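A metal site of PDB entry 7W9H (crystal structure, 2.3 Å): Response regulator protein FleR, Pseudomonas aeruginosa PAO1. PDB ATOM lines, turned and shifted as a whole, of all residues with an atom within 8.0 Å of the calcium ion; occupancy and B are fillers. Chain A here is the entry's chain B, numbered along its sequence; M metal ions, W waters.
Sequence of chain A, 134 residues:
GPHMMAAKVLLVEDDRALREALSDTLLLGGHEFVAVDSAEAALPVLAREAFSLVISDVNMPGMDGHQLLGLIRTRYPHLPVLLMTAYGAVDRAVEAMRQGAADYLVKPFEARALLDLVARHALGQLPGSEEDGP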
ATOM      1  N   VAL A  12      15.543   6.136 -11.899  1.00  0.00           N
ATOM      2  CA  VAL A  12      14.326   6.341 -11.123  1.00  0.00           C
ATOM      3  C   VAL A  12      14.323   5.265 -10.057  1.00  0.00           C
ATOM      4  O   VAL A  12      13.976   4.110 -10.335  1.00  0.00           O
ATOM      5  CB  VAL A  12      13.058   6.274 -11.967  1.00  0.00           C
ATOM      6  CG1 VAL A  12      11.828   6.599 -11.101  1.00  0.00           C
ATOM      7  CG2 VAL A  12      13.169   7.187 -13.163  1.00  0.00           C
ATOM      8  N   GLU A  13      14.690   5.633  -8.828  1.00  0.00           N
ATOM      9  CA  GLU A  13      14.763   4.674  -7.739  1.00  0.00           C
ATOM     10  C   GLU A  13      14.436   5.383  -6.429  1.00  0.00           C
ATOM     11  O   GLU A  13      15.077   6.377  -6.086  1.00  0.00           O
ATOM     12  CB  GLU A  13      16.153   4.032  -7.670  1.00  0.00           C
ATOM     13  CG  GLU A  13      16.349   3.114  -6.465  1.00  0.00           C
ATOM     14  CD  GLU A  13      15.369   1.937  -6.422  1.00  0.00           C
ATOM     15  OE1 GLU A  13      14.338   2.016  -5.695  1.00  0.00           O
ATOM     16  OE2 GLU A  13      15.647   0.916  -7.085  1.00  0.00           O
ATOM     17  N   ASP A  14      13.450   4.853  -5.715  1.00  0.00           N
ATOM     18  CA  ASP A  14      13.000   5.493  -4.474  1.00  0.00           C
ATOM     19  C   ASP A  14      13.838   5.090  -3.267  1.00  0.00           C
ATOM     20  O   ASP A  14      13.940   5.875  -2.313  1.00  0.00           O
ATOM     21  CB  ASP A  14      11.534   5.171  -4.225  1.00  0.00           C
ATOM     22  CG  ASP A  14      11.234   3.684  -4.279  1.00  0.00           C
ATOM     23  OD1 ASP A  14      11.704   3.005  -5.220  1.00  0.00           O
ATOM     24  OD2 ASP A  14      10.530   3.188  -3.369  1.00  0.00           O
ATOM     25  N   ASP A  15      14.434   3.896  -3.247  1.00  0.00           N
ATOM     26  CA  ASP A  15      15.357   3.541  -2.168  1.00  0.00           C
ATOM     27  C   ASP A  15      16.653   4.339  -2.322  1.00  0.00           C
ATOM     28  O   ASP A  15      17.446   4.070  -3.248  1.00  0.00           O
ATOM     29  CB  ASP A  15      15.621   2.040  -2.188  1.00  0.00           C
ATOM     30  CG  ASP A  15      16.669   1.596  -1.156  1.00  0.00           C
ATOM     31  OD1 ASP A  15      16.311   0.927  -0.160  1.00  0.00           O
ATOM     32  OD2 ASP A  15      17.867   1.902  -1.355  1.00  0.00           O
ATOM     33  N   LEU A  18      20.070   2.284  -2.663  1.00  0.00           N
ATOM     34  CA  LEU A  18      20.288   1.719  -3.998  1.00  0.00           C
ATOM     35  C   LEU A  18      20.514   2.802  -5.048  1.00  0.00           C
ATOM     36  O   LEU A  18      21.372   2.645  -5.931  1.00  0.00           O
ATOM     37  CB  LEU A  18      19.116   0.831  -4.388  1.00  0.00           C
ATOM     38  CG  LEU A  18      19.247   0.093  -5.725  1.00  0.00           C
ATOM     39  CD1 LEU A  18      20.517  -0.755  -5.779  1.00  0.00           C
ATOM     40  CD2 LEU A  18      18.030  -0.772  -5.912  1.00  0.00           C
ATOM     41  N   ASP A  37      13.605  10.114  -7.502  1.00  0.00           N
ATOM     42  CA  ASP A  37      13.116   9.150  -6.531  1.00  0.00           C
ATOM     43  C   ASP A  37      11.724   8.635  -6.835  1.00  0.00           C
ATOM     44  O   ASP A  37      11.207   7.811  -6.087  1.00  0.00           O
ATOM     45  CB  ASP A  37      13.148   9.758  -5.113  1.00  0.00           C
ATOM     46  CG  ASP A  37      12.261  10.989  -4.973  1.00  0.00           C
ATOM     47  OD1 ASP A  37      12.415  11.693  -3.958  1.00  0.00           O
ATOM     48  OD2 ASP A  37      11.395  11.262  -5.828  1.00  0.00           O
ATOM     49  N   ASP A  57      12.774   1.574 -11.102  1.00  0.00           N
ATOM     50  CA  ASP A  57      12.134   0.627 -10.199  1.00  0.00           C
ATOM     51  C   ASP A  57      10.651   0.472 -10.553  1.00  0.00           C
ATOM     52  O   ASP A  57      10.042   1.353 -11.141  1.00  0.00           O
ATOM     53  CB  ASP A  57      12.305   1.096  -8.753  1.00  0.00           C
ATOM     54  CG  ASP A  57      11.757   0.104  -7.750  1.00  0.00           C
ATOM     55  OD1 ASP A  57      11.811  -1.105  -8.031  1.00  0.00           O
ATOM     56  OD2 ASP A  57      11.268   0.524  -6.689  1.00  0.00           O
ATOM     57  N   VAL A  58      10.078  -0.677 -10.215  1.00  0.00           N
ATOM     58  CA  VAL A  58       8.673  -0.923 -10.538  1.00  0.00           C
ATOM     59  C   VAL A  58       7.745  -0.443  -9.426  1.00  0.00           C
ATOM     60  O   VAL A  58       6.760   0.263  -9.671  1.00  0.00           O
ATOM     61  CB  VAL A  58       8.433  -2.418 -10.874  1.00  0.00           C
ATOM     62  CG1 VAL A  58       6.947  -2.743 -10.839  1.00  0.00           C
ATOM     63  CG2 VAL A  58       9.030  -2.769 -12.241  1.00  0.00           C
ATOM     64  N   ASN A  59       8.046  -0.755  -8.167  1.00  0.00           N
ATOM     65  CA  ASN A  59       7.133  -0.489  -7.057  1.00  0.00           C
ATOM     66  C   ASN A  59       7.533   0.799  -6.339  1.00  0.00           C
ATOM     67  O   ASN A  59       8.566   0.852  -5.685  1.00  0.00           O
ATOM     68  CB  ASN A  59       7.125  -1.684  -6.112  1.00  0.00           C
ATOM     69  CG  ASN A  59       6.880  -2.967  -6.841  1.00  0.00           C
ATOM     70  OD1 ASN A  59       5.738  -3.287  -7.179  1.00  0.00           O
ATOM     71  ND2 ASN A  59       7.954  -3.698  -7.142  1.00  0.00           N
ATOM     72  N   MET A  60       6.705   1.823  -6.462  1.00  0.00           N
ATOM     73  CA  MET A  60       7.113   3.123  -5.954  1.00  0.00           C
ATOM     74  C   MET A  60       5.974   3.793  -5.190  1.00  0.00           C
ATOM     75  O   MET A  60       4.864   3.252  -5.165  1.00  0.00           O
ATOM     76  CB  MET A  60       7.629   3.959  -7.137  1.00  0.00           C
ATOM     77  CG  MET A  60       9.020   3.545  -7.570  1.00  0.00           C
ATOM     78  SD  MET A  60       9.634   4.492  -8.941  1.00  0.00           S
ATOM     79  CE  MET A  60       8.162   4.564  -9.989  1.00  0.00           C
ATOM     80  N   PRO A  61       6.201   4.944  -4.504  1.00  0.00           N
ATOM     81  CA  PRO A  61       5.126   5.525  -3.669  1.00  0.00           C
ATOM     82  C   PRO A  61       3.887   5.882  -4.463  1.00  0.00           C
ATOM     83  O   PRO A  61       2.783   5.426  -4.161  1.00  0.00           O
ATOM     84  CB  PRO A  61       5.782   6.776  -3.082  1.00  0.00           C
ATOM     85  CG  PRO A  61       6.845   7.130  -4.103  1.00  0.00           C
ATOM     86  CD  PRO A  61       7.404   5.796  -4.463  1.00  0.00           C
ATOM     87  N   ASP A  64       3.498   3.707 -10.529  1.00  0.00           N
ATOM     88  CA  ASP A  64       4.436   2.592 -10.605  1.00  0.00           C
ATOM     89  C   ASP A  64       5.125   2.540 -11.970  1.00  0.00           C
ATOM     90  O   ASP A  64       4.739   3.214 -12.922  1.00  0.00           O
ATOM     91  CB  ASP A  64       3.716   1.281 -10.303  1.00  0.00           C
ATOM     92  CG  ASP A  64       3.753   0.951  -8.832  1.00  0.00           C
ATOM     93  OD1 ASP A  64       4.440   1.689  -8.091  1.00  0.00           O
ATOM     94  OD2 ASP A  64       3.116  -0.027  -8.420  1.00  0.00           O
ATOM     95  N   MET A  84      13.313  -2.427 -13.219  1.00  0.00           N
ATOM     96  CA  MET A  84      13.949  -3.252 -12.193  1.00  0.00           C
ATOM     97  C   MET A  84      13.004  -3.407 -11.011  1.00  0.00           C
ATOM     98  O   MET A  84      12.195  -2.523 -10.719  1.00  0.00           O
ATOM     99  CB  MET A  84      15.298  -2.657 -11.727  1.00  0.00           C
ATOM    100  CG  MET A  84      15.187  -1.280 -11.118  1.00  0.00           C
ATOM    101  SD  MET A  84      16.799  -0.503 -10.789  1.00  0.00           S
ATOM    102  CE  MET A  84      16.227   1.149 -10.359  1.00  0.00           C
ATOM    103  N   THR A  85      13.065  -4.556 -10.348  1.00  0.00           N
ATOM    104  CA  THR A  85      12.104  -4.819  -9.295  1.00  0.00           C
ATOM    105  C   THR A  85      12.737  -5.729  -8.263  1.00  0.00           C
ATOM    106  O   THR A  85      13.597  -6.556  -8.583  1.00  0.00           O
ATOM    107  CB  THR A  85      10.785  -5.414  -9.861  1.00  0.00           C
ATOM    108  OG1 THR A  85       9.844  -5.581  -8.802  1.00  0.00           O
ATOM    109  CG2 THR A  85      10.999  -6.758 -10.539  1.00  0.00           C
ATOM    110  N   ALA A  86      12.350  -5.501  -7.004  1.00  0.00           N
ATOM    111  CA  ALA A  86      12.703  -6.417  -5.930  1.00  0.00           C
ATOM    112  C   ALA A  86      11.886  -7.696  -6.075  1.00  0.00           C
ATOM    113  O   ALA A  86      12.409  -8.803  -5.914  1.00  0.00           O
ATOM    114  CB  ALA A  86      12.442  -5.750  -4.582  1.00  0.00           C
ATOM    115  N   TYR A  87      10.605  -7.551  -6.399  1.00  0.00           N
ATOM    116  CA  TYR A  87       9.692  -8.702  -6.571  1.00  0.00           C
ATOM    117  C   TYR A  87       9.272  -8.812  -8.026  1.00  0.00           C
ATOM    118  O   TYR A  87       8.565  -7.999  -8.510  1.00  0.00           O
ATOM    119  CB  TYR A  87       8.424  -8.579  -5.730  1.00  0.00           C
ATOM    120  CG  TYR A  87       8.362  -7.364  -4.860  1.00  0.00           C
ATOM    121  CD1 TYR A  87       9.115  -7.280  -3.712  1.00  0.00           C
ATOM    122  CD2 TYR A  87       7.566  -6.294  -5.187  1.00  0.00           C
ATOM    123  CE1 TYR A  87       9.090  -6.162  -2.906  1.00  0.00           C
ATOM    124  CE2 TYR A  87       7.517  -5.158  -4.389  1.00  0.00           C
ATOM    125  CZ  TYR A  87       8.295  -5.086  -3.262  1.00  0.00           C
ATOM    126  OH  TYR A  87       8.285  -3.982  -2.477  1.00  0.00           O
ATOM    127  N   LYS A 107      16.207  -7.568  -8.871  1.00  0.00           N
ATOM    128  CA  LYS A 107      17.344  -7.140  -8.080  1.00  0.00           C
ATOM    129  C   LYS A 107      17.830  -8.269  -7.183  1.00  0.00           C
ATOM    130  O   LYS A 107      17.070  -9.174  -6.819  1.00  0.00           O
ATOM    131  CB  LYS A 107      16.964  -5.921  -7.219  1.00  0.00           C
ATOM    132  CG  LYS A 107      16.608  -4.649  -7.973  1.00  0.00           C
ATOM    133  CD  LYS A 107      15.954  -3.644  -6.992  1.00  0.00           C
ATOM    134  CE  LYS A 107      15.210  -2.547  -7.707  1.00  0.00           C
ATOM    135  NZ  LYS A 107      14.508  -1.655  -6.737  1.00  0.00           N
HETATM  136 CA    CA M   1      10.623   0.878  -4.422  1.00  0.00          CA
HETATM  137  O   HOH W   1      12.952   0.239  -4.424  1.00  0.00           O
HETATM  138  O   HOH W   2      10.970  -1.346  -4.176  1.00  0.00           O
HETATM  139  O   HOH W   3       9.586   0.200  -2.344  1.00  0.00           O
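The calcium ion is bound by water W2.
The side-chain carboxylate (OD2) of Asp 57 is bound to the calcium ion, at 2.4 Å.
O of Asn 59 binds the calcium ion (2.4 Å).
Water W1 is bound to the calcium ion (2.4 Å).
The calcium ion is bound by water W3 (2.4 Å).
OD1 of Asp 14 is bound to the calcium ion (2.5 Å).
The calcium ion is bound by OD2 of Asp 14 (2.5 Å).
The calcium ion has seven donor atoms within binding distance.
OG1 of Thr 85 sits at hydrogen-bond distance from ND2 of Asn 59, at 3.1 Å.
OD1 of Asp 57 lies within salt-bridge range of NZ of Lys 107 (3.0 Å).
The backbone carbonyl oxygen (O) of Val 12 lies within hydrogen-bond range of the backbone NH (N) of Asp 57 (2.9 Å).
Water W1 bridges OE1 of Glu 13 and NZ of Lys 107.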
